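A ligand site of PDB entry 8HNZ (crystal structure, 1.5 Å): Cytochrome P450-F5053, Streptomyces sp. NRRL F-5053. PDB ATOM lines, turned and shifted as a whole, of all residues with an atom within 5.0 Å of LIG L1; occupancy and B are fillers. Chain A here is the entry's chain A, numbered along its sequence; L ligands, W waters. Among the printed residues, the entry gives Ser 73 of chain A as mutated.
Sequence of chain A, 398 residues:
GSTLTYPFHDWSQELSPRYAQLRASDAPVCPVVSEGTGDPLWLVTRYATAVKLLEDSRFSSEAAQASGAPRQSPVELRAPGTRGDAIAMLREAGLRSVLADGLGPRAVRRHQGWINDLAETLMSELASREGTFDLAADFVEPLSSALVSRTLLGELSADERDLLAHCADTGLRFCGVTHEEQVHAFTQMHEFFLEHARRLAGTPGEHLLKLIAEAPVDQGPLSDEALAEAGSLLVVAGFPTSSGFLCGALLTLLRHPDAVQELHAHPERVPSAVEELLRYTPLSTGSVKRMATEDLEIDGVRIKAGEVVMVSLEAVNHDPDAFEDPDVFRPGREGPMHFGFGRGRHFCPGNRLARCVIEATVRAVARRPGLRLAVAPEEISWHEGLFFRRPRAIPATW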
ATOM      1  N   GLN A  72      -2.019  13.853  -8.357  1.00  0.00           N
ATOM      2  CA  GLN A  72      -2.116  14.031  -6.913  1.00  0.00           C
ATOM      3  C   GLN A  72      -0.969  14.875  -6.342  1.00  0.00           C
ATOM      4  O   GLN A  72      -1.127  15.459  -5.257  1.00  0.00           O
ATOM      5  CB  GLN A  72      -2.167  12.664  -6.222  1.00  0.00           C
ATOM      6  CG  GLN A  72      -0.861  11.932  -6.308  1.00  0.00           C
ATOM      7  CD  GLN A  72      -1.014  10.449  -6.011  1.00  0.00           C
ATOM      8  OE1 GLN A  72      -1.118  10.030  -4.853  1.00  0.00           O
ATOM      9  NE2 GLN A  72      -0.997   9.638  -7.066  1.00  0.00           N
ATOM     10  N   SER A  73       0.181  14.956  -7.024  1.00  0.00           N
ATOM     11  CA  SER A  73       1.317  15.757  -6.598  1.00  0.00           C
ATOM     12  C   SER A  73       1.068  17.242  -6.871  1.00  0.00           C
ATOM     13  O   SER A  73       0.483  17.576  -7.912  1.00  0.00           O
ATOM     14  CB  SER A  73       2.586  15.324  -7.337  1.00  0.00           C
ATOM     15  OG  SER A  73       3.666  16.175  -6.981  1.00  0.00           O
ATOM     16  N   LEU A  77       6.572  15.586 -11.411  1.00  0.00           N
ATOM     17  CA  LEU A  77       7.716  14.858 -10.873  1.00  0.00           C
ATOM     18  C   LEU A  77       8.784  14.673 -11.953  1.00  0.00           C
ATOM     19  O   LEU A  77       9.145  13.555 -12.346  1.00  0.00           O
ATOM     20  CB  LEU A  77       7.257  13.510 -10.328  1.00  0.00           C
ATOM     21  CG  LEU A  77       6.168  13.573  -9.239  1.00  0.00           C
ATOM     22  CD1 LEU A  77       5.839  12.152  -8.735  1.00  0.00           C
ATOM     23  CD2 LEU A  77       6.576  14.517  -8.068  1.00  0.00           C
ATOM     24  N   PHE A 174       3.953  16.103  -0.687  1.00  0.00           N
ATOM     25  CA  PHE A 174       2.635  16.686  -0.862  1.00  0.00           C
ATOM     26  C   PHE A 174       2.568  18.112  -0.342  1.00  0.00           C
ATOM     27  O   PHE A 174       1.722  18.889  -0.796  1.00  0.00           O
ATOM     28  CB  PHE A 174       1.574  15.836  -0.156  1.00  0.00           C
ATOM     29  CG  PHE A 174       1.193  14.603  -0.911  1.00  0.00           C
ATOM     30  CD1 PHE A 174       0.484  14.718  -2.093  1.00  0.00           C
ATOM     31  CD2 PHE A 174       1.512  13.330  -0.408  1.00  0.00           C
ATOM     32  CE1 PHE A 174       0.123  13.593  -2.799  1.00  0.00           C
ATOM     33  CE2 PHE A 174       1.138  12.195  -1.118  1.00  0.00           C
ATOM     34  CZ  PHE A 174       0.438  12.321  -2.304  1.00  0.00           C
ATOM     35  N   ALA A 237      13.061   6.050  -7.071  1.00  0.00           N
ATOM     36  CA  ALA A 237      12.437   4.741  -6.868  1.00  0.00           C
ATOM     37  C   ALA A 237      13.153   3.930  -5.798  1.00  0.00           C
ATOM     38  O   ALA A 237      12.524   3.072  -5.167  1.00  0.00           O
ATOM     39  CB  ALA A 237      12.413   3.930  -8.176  1.00  0.00           C
ATOM     40  N   THR A 241      12.219   5.278  -0.778  1.00  0.00           N
ATOM     41  CA  THR A 241      11.401   4.091  -0.576  1.00  0.00           C
ATOM     42  C   THR A 241      12.080   3.125   0.350  1.00  0.00           C
ATOM     43  O   THR A 241      11.511   2.702   1.360  1.00  0.00           O
ATOM     44  CB  THR A 241      11.135   3.432  -1.926  1.00  0.00           C
ATOM     45  OG1 THR A 241      12.401   3.266  -2.577  1.00  0.00           O
ATOM     46  CG2 THR A 241      10.247   4.346  -2.780  1.00  0.00           C
ATOM     47  N   LEU A 283       3.864   2.597   3.700  1.00  0.00           N
ATOM     48  CA  LEU A 283       4.962   3.372   3.132  1.00  0.00           C
ATOM     49  C   LEU A 283       4.433   4.642   2.484  1.00  0.00           C
ATOM     50  O   LEU A 283       4.608   5.735   3.042  1.00  0.00           O
ATOM     51  CB  LEU A 283       5.759   2.541   2.125  1.00  0.00           C
ATOM     52  CG  LEU A 283       6.977   3.261   1.556  1.00  0.00           C
ATOM     53  CD1 LEU A 283       7.943   3.763   2.638  1.00  0.00           C
ATOM     54  CD2 LEU A 283       7.679   2.408   0.522  1.00  0.00           C
ATOM     55  N   SER A 284       3.794   4.548   1.338  1.00  0.00           N
ATOM     56  CA  SER A 284       3.399   5.767   0.635  1.00  0.00           C
ATOM     57  C   SER A 284       2.182   6.415   1.291  1.00  0.00           C
ATOM     58  O   SER A 284       1.267   5.733   1.767  1.00  0.00           O
ATOM     59  CB  SER A 284       3.111   5.442  -0.834  1.00  0.00           C
ATOM     60  OG  SER A 284       2.665   6.607  -1.509  1.00  0.00           O
ATOM     61  N   THR A 285       2.196   7.747   1.336  1.00  0.00           N
ATOM     62  CA  THR A 285       1.034   8.508   1.778  1.00  0.00           C
ATOM     63  C   THR A 285       0.110   8.873   0.633  1.00  0.00           C
ATOM     64  O   THR A 285      -0.948   9.468   0.874  1.00  0.00           O
ATOM     65  CB  THR A 285       1.466   9.785   2.505  1.00  0.00           C
ATOM     66  OG1 THR A 285       2.229  10.601   1.600  1.00  0.00           O
ATOM     67  CG2 THR A 285       2.304   9.462   3.746  1.00  0.00           C
ATOM     68  N   GLY A 286       0.506   8.577  -0.605  1.00  0.00           N
ATOM     69  CA  GLY A 286      -0.357   8.674  -1.756  1.00  0.00           C
ATOM     70  C   GLY A 286      -0.723   7.313  -2.338  1.00  0.00           C
ATOM     71  O   GLY A 286      -0.784   6.305  -1.621  1.00  0.00           O
ATOM     72  N   SER A 287      -0.947   7.285  -3.640  1.00  0.00           N
ATOM     73  CA  SER A 287      -1.510   6.119  -4.300  1.00  0.00           C
ATOM     74  C   SER A 287      -0.820   5.860  -5.625  1.00  0.00           C
ATOM     75  O   SER A 287      -0.386   6.802  -6.304  1.00  0.00           O
ATOM     76  CB  SER A 287      -3.025   6.296  -4.544  1.00  0.00           C
ATOM     77  OG  SER A 287      -3.757   6.339  -3.338  1.00  0.00           O
ATOM     78  N   VAL A 288      -0.720   4.579  -5.988  1.00  0.00           N
ATOM     79  CA  VAL A 288      -0.420   4.236  -7.380  1.00  0.00           C
ATOM     80  C   VAL A 288      -1.588   4.717  -8.232  1.00  0.00           C
ATOM     81  O   VAL A 288      -2.731   4.806  -7.757  1.00  0.00           O
ATOM     82  CB  VAL A 288      -0.160   2.736  -7.632  1.00  0.00           C
ATOM     83  CG1 VAL A 288       0.942   2.190  -6.743  1.00  0.00           C
ATOM     84  CG2 VAL A 288      -1.428   1.903  -7.487  1.00  0.00           C
ATOM     85  N   LYS A 289      -1.330   5.068  -9.491  1.00  0.00           N
ATOM     86  CA  LYS A 289      -2.402   5.689 -10.257  1.00  0.00           C
ATOM     87  C   LYS A 289      -2.280   5.394 -11.753  1.00  0.00           C
ATOM     88  O   LYS A 289      -1.201   5.083 -12.265  1.00  0.00           O
ATOM     89  CB  LYS A 289      -2.469   7.207  -9.989  1.00  0.00           C
ATOM     90  CG  LYS A 289      -1.482   8.065 -10.721  1.00  0.00           C
ATOM     91  CD  LYS A 289      -0.031   7.759 -10.363  1.00  0.00           C
ATOM     92  CE  LYS A 289       0.917   8.789 -10.942  1.00  0.00           C
ATOM     93  NZ  LYS A 289       2.323   8.320 -10.780  1.00  0.00           N
ATOM     94  N   LEU A 313      -2.214   1.465  -1.842  1.00  0.00           N
ATOM     95  CA  LEU A 313      -1.694   0.166  -1.455  1.00  0.00           C
ATOM     96  C   LEU A 313      -1.916  -0.113   0.017  1.00  0.00           C
ATOM     97  O   LEU A 313      -2.201  -1.246   0.409  1.00  0.00           O
ATOM     98  CB  LEU A 313      -0.207   0.085  -1.792  1.00  0.00           C
ATOM     99  CG  LEU A 313       0.137   0.379  -3.252  1.00  0.00           C
ATOM    100  CD1 LEU A 313       1.634   0.160  -3.426  1.00  0.00           C
ATOM    101  CD2 LEU A 313      -0.699  -0.399  -4.300  1.00  0.00           C
ATOM    102  N   GLY A 340       2.399  -4.582  -1.398  1.00  0.00           N
ATOM    103  CA  GLY A 340       3.453  -3.642  -1.037  1.00  0.00           C
ATOM    104  C   GLY A 340       4.366  -3.278  -2.200  1.00  0.00           C
ATOM    105  O   GLY A 340       5.015  -2.229  -2.169  1.00  0.00           O
ATOM    106  N   PHE A 387       5.916  11.842   0.304  1.00  0.00           N
ATOM    107  CA  PHE A 387       5.274  10.713  -0.367  1.00  0.00           C
ATOM    108  C   PHE A 387       5.541   9.408   0.362  1.00  0.00           C
ATOM    109  O   PHE A 387       4.668   8.527   0.405  1.00  0.00           O
ATOM    110  CB  PHE A 387       5.801  10.563  -1.804  1.00  0.00           C
ATOM    111  CG  PHE A 387       5.406  11.682  -2.740  1.00  0.00           C
ATOM    112  CD1 PHE A 387       4.462  12.648  -2.395  1.00  0.00           C
ATOM    113  CD2 PHE A 387       5.960  11.696  -4.028  1.00  0.00           C
ATOM    114  CE1 PHE A 387       4.096  13.647  -3.316  1.00  0.00           C
ATOM    115  CE2 PHE A 387       5.611  12.697  -4.958  1.00  0.00           C
ATOM    116  CZ  PHE A 387       4.681  13.692  -4.586  1.00  0.00           C
ATOM    117  N   PHE A 388       6.754   9.215   0.883  1.00  0.00           N
ATOM    118  CA  PHE A 388       7.116   7.958   1.523  1.00  0.00           C
ATOM    119  C   PHE A 388       7.450   8.244   2.987  1.00  0.00           C
ATOM    120  O   PHE A 388       8.475   8.856   3.277  1.00  0.00           O
ATOM    121  CB  PHE A 388       8.266   7.271   0.766  1.00  0.00           C
ATOM    122  CG  PHE A 388       7.984   7.088  -0.714  1.00  0.00           C
ATOM    123  CD1 PHE A 388       6.977   6.232  -1.123  1.00  0.00           C
ATOM    124  CD2 PHE A 388       8.671   7.834  -1.681  1.00  0.00           C
ATOM    125  CE1 PHE A 388       6.670   6.092  -2.462  1.00  0.00           C
ATOM    126  CE2 PHE A 388       8.382   7.674  -3.030  1.00  0.00           C
ATOM    127  CZ  PHE A 388       7.364   6.808  -3.421  1.00  0.00           C
HETATM  128  C1  LIG L   1       3.042   7.553  -7.023  1.00  0.00           C
HETATM  129  C2  LIG L   1       3.496   9.312  -5.433  1.00  0.00           C
HETATM  130  C3  LIG L   1       2.690  10.753  -5.273  1.00  0.00           C
HETATM  131  C4  LIG L   1       2.662  11.280  -6.709  1.00  0.00           C
HETATM  132  C5  LIG L   1       2.754  10.171  -7.549  1.00  0.00           C
HETATM  133  C6  LIG L   1       3.165   8.458  -4.200  1.00  0.00           C
HETATM  134  C7  LIG L   1       3.445   6.567  -5.915  1.00  0.00           C
HETATM  135  C8  LIG L   1       2.917   5.153  -6.162  1.00  0.00           C
HETATM  136  C9  LIG L   1       3.228   4.286  -4.919  1.00  0.00           C
HETATM  137  C10 LIG L   1       2.338   3.862  -3.944  1.00  0.00           C
HETATM  138  C11 LIG L   1       4.355   3.149  -3.353  1.00  0.00           C
HETATM  139  C12 LIG L   1       5.475   2.566  -2.719  1.00  0.00           C
HETATM  140  C13 LIG L   1       6.746   2.697  -3.285  1.00  0.00           C
HETATM  141  C14 LIG L   1       6.894   3.361  -4.497  1.00  0.00           C
HETATM  142  C15 LIG L   1       5.801   3.955  -5.124  1.00  0.00           C
HETATM  143  C16 LIG L   1       4.517   3.833  -4.539  1.00  0.00           C
HETATM  144  F1  LIG L   1       8.116   3.500  -5.069  1.00  0.00           F
HETATM  145  N1  LIG L   1       3.104   8.870  -6.614  1.00  0.00           N
HETATM  146  N2  LIG L   1       3.120   6.987  -4.496  1.00  0.00           N
HETATM  147  N3  LIG L   1       3.030   3.188  -3.041  1.00  0.00           N
HETATM  148  O1  LIG L   1       2.708   7.229  -8.107  1.00  0.00           O
HETATM  149  O2  LIG L   1       2.970   8.879  -3.099  1.00  0.00           O
HETATM  150  C1  LG2 L   2       5.686   6.934 -11.268  1.00  0.00           C
HETATM  151  C2  LG2 L   2       7.945   6.984 -12.196  1.00  0.00           C
HETATM  152  C3  LG2 L   2       9.120   7.547 -11.186  1.00  0.00           C
HETATM  153  C4  LG2 L   2       8.600   8.975 -10.913  1.00  0.00           C
HETATM  154  C5  LG2 L   2       7.338   9.089 -11.488  1.00  0.00           C
HETATM  155  C6  LG2 L   2       8.000   5.465 -12.446  1.00  0.00           C
HETATM  156  C7  LG2 L   2       5.591   5.435 -11.454  1.00  0.00           C
HETATM  157  C8  LG2 L   2       5.404   4.900 -10.032  1.00  0.00           C
HETATM  158  C9  LG2 L   2       6.638   5.040  -9.112  1.00  0.00           C
HETATM  159  C10 LG2 L   2       7.610   4.068  -8.884  1.00  0.00           C
HETATM  160  C11 LG2 L   2       8.169   5.828  -7.655  1.00  0.00           C
HETATM  161  C12 LG2 L   2       8.814   6.756  -6.759  1.00  0.00           C
HETATM  162  C13 LG2 L   2       8.253   7.995  -6.559  1.00  0.00           C
HETATM  163  C14 LG2 L   2       7.068   8.306  -7.220  1.00  0.00           C
HETATM  164  C15 LG2 L   2       6.435   7.428  -8.088  1.00  0.00           C
HETATM  165  C16 LG2 L   2       7.001   6.149  -8.303  1.00  0.00           C
HETATM  166  F1  LG2 L   2       6.495   9.515  -7.026  1.00  0.00           F
HETATM  167  N1  LG2 L   2       6.899   7.504 -11.641  1.00  0.00           N
HETATM  168  N2  LG2 L   2       6.759   4.703 -12.084  1.00  0.00           N
HETATM  169  N3  LG2 L   2       8.511   4.547  -8.019  1.00  0.00           N
HETATM  170  O1  LG2 L   2       4.820   7.565 -10.767  1.00  0.00           O
HETATM  171  O2  LG2 L   2       8.936   4.885 -12.917  1.00  0.00           O
HETATM  172  C1  LG3 L   3       7.763   0.598  -8.877  1.00  0.00           C
HETATM  173  C2  LG3 L   3      12.584   0.343  -8.677  1.00  0.00           C
HETATM  174  C3  LG3 L   3      12.344  -0.272  -3.892  1.00  0.00           C
HETATM  175  C4  LG3 L   3       7.539  -0.335  -4.143  1.00  0.00           C
HETATM  176  C5  LG3 L   3       9.090   0.690  -9.211  1.00  0.00           C
HETATM  177  C6  LG3 L   3       9.616   1.123 -10.496  1.00  0.00           C
HETATM  178  C7  LG3 L   3      10.945   1.047 -10.442  1.00  0.00           C
HETATM  179  C8  LG3 L   3      11.309   0.591  -9.139  1.00  0.00           C
HETATM  180  C9  LG3 L   3      11.942   1.413 -11.561  1.00  0.00           C
HETATM  181  C10 LG3 L   3       8.759   1.634 -11.687  1.00  0.00           C
HETATM  182  C11 LG3 L   3       8.168   0.481 -12.435  1.00  0.00           C
HETATM  183  C12 LG3 L   3       7.104   0.873 -13.418  1.00  0.00           C
HETATM  184  O1  LG3 L   3       6.899   0.066 -14.357  1.00  0.00           O
HETATM  185  O2  LG3 L   3       6.511   1.963 -13.272  1.00  0.00           O
HETATM  186  C13 LG3 L   3      12.910   0.116  -7.370  1.00  0.00           C
HETATM  187  C14 LG3 L   3      14.268  -0.040  -6.874  1.00  0.00           C
HETATM  188  C15 LG3 L   3      14.206  -0.185  -5.549  1.00  0.00           C
HETATM  189  C16 LG3 L   3      12.813  -0.152  -5.175  1.00  0.00           C
HETATM  190  C17 LG3 L   3      15.534  -0.005  -7.762  1.00  0.00           C
HETATM  191  C18 LG3 L   3      15.344  -0.423  -4.559  1.00  0.00           C
HETATM  192  C19 LG3 L   3      16.378  -1.227  -4.848  1.00  0.00           C
HETATM  193  C20 LG3 L   3      11.020  -0.315  -3.548  1.00  0.00           C
HETATM  194  C21 LG3 L   3      10.523  -0.529  -2.205  1.00  0.00           C
HETATM  195  C22 LG3 L   3       9.184  -0.554  -2.267  1.00  0.00           C
HETATM  196  C23 LG3 L   3       8.825  -0.364  -3.637  1.00  0.00           C
HETATM  197  C24 LG3 L   3      11.460  -0.677  -0.971  1.00  0.00           C
HETATM  198  C25 LG3 L   3       8.130  -0.760  -1.170  1.00  0.00           C
HETATM  199  C26 LG3 L   3       8.430  -1.038   0.105  1.00  0.00           C
HETATM  200  C27 LG3 L   3       7.232  -0.107  -5.438  1.00  0.00           C
HETATM  201  C28 LG3 L   3       5.865  -0.062  -5.943  1.00  0.00           C
HETATM  202  C29 LG3 L   3       5.902   0.152  -7.263  1.00  0.00           C
HETATM  203  C30 LG3 L   3       7.306   0.289  -7.617  1.00  0.00           C
HETATM  204  C31 LG3 L   3       4.605  -0.276  -5.085  1.00  0.00           C
HETATM  205  C32 LG3 L   3       4.675   0.224  -8.206  1.00  0.00           C
HETATM  206  C33 LG3 L   3       4.218   1.634  -8.570  1.00  0.00           C
HETATM  207  C34 LG3 L   3       3.051   1.549  -9.527  1.00  0.00           C
HETATM  208  O3  LG3 L   3       2.366   0.503  -9.641  1.00  0.00           O
HETATM  209  O4  LG3 L   3       2.793   2.562 -10.198  1.00  0.00           O
HETATM  210  N1  LG3 L   3      10.150   0.396  -8.384  1.00  0.00           N
HETATM  211  N2  LG3 L   3      12.047   0.028  -6.288  1.00  0.00           N
HETATM  212  N3  LG3 L   3       9.963  -0.219  -4.414  1.00  0.00           N
HETATM  213  N4  LG3 L   3       8.097   0.149  -6.495  1.00  0.00           N
HETATM  214 FE1  LG3 L   3      10.073   0.028  -6.387  1.00  0.00          FE
HETATM  215  O   HOH W   1       3.056   2.226  -0.251  1.00  0.00           O
HETATM  216  O   HOH W   2      10.151   2.130  -6.258  1.00  0.00           O
HETATM  217  O   HOH W   3      -0.162   3.615  -1.808  1.00  0.00           O
HETATM  218  O   HOH W   4       1.799   4.930  -9.690  1.00  0.00           O
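A nitrogen (N2) of LG2 L2 is in hydrogen-bond range of an oxygen (O2) of LG3 L3 (3.0 Å).
Merely in contact with LIG L1: Thr 241 (3.2 Å), Leu 313 (3.4 Å), Phe 388 (3.4 Å), Gly 286 (3.5 Å), Phe 387 (3.5 Å), Val 288 (3.5 Å), Ser 287 (3.6 Å), Gln 72 (3.6 Å), Leu 77 (3.9 Å) and Leu 283 (3.9 Å).
Hydrophobic or aromatic side chains within 4 Å of LIG L1: Leu 77, Leu 283, Val 288, Leu 313, Phe 387 and Phe 388.
12 residues have an atom within 4 Å of LIG L1: Gln 72, Leu 77, Thr 241, Leu 283, Ser 284, Gly 286, Ser 287, Val 288, Lys 289, Leu 313, Phe 387 and Phe 388.
Along chain A the residues within 4 Å of LIG L1 span positions 72 to 388.
N of Gly 286 is in hydrogen-bond range of OG of Ser 284 (3.1 Å).
OG of Ser 284 sits close to O of Phe 387 (3.4 Å).
The backbone carbonyl oxygen (O) of Ala 237 sits at hydrogen-bond distance from the side-chain hydroxyl (OG1) of Thr 241.
The backbone carbonyl oxygen of Phe 387 is in hydrogen-bond range of the backbone NH of Thr 285 (2.8 Å).
O of Ser 287 lies within hydrogen-bond range of NE2 of Gln 72 (3.0 Å).
An oxygen (O2) of LIG L1 sits at hydrogen-bond distance from the side-chain hydroxyl (OG) of Ser 284.
O1 of LIG L1 is in hydrogen-bond range of NZ of Lys 289 (2.9 Å).
NZ of Lys 289 lies within hydrogen-bond range of O1 of LG2 L2.
Water W2 bridges O of Ala 237 and N3 of LG2 L2.
Water W4 lies within hydrogen-bond range of an oxygen (O4) of LG3 L3 (2.6 Å), an oxygen (O1) of LIG L1 (2.9 Å) and the backbone NH of Lys 289 (3.1 Å).
Water W1 bridges N of Ser 284 and N3 of LIG L1.
Water W3 lies within hydrogen-bond range of O of Gly 286, N of Leu 313 and N3 of LIG L1.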
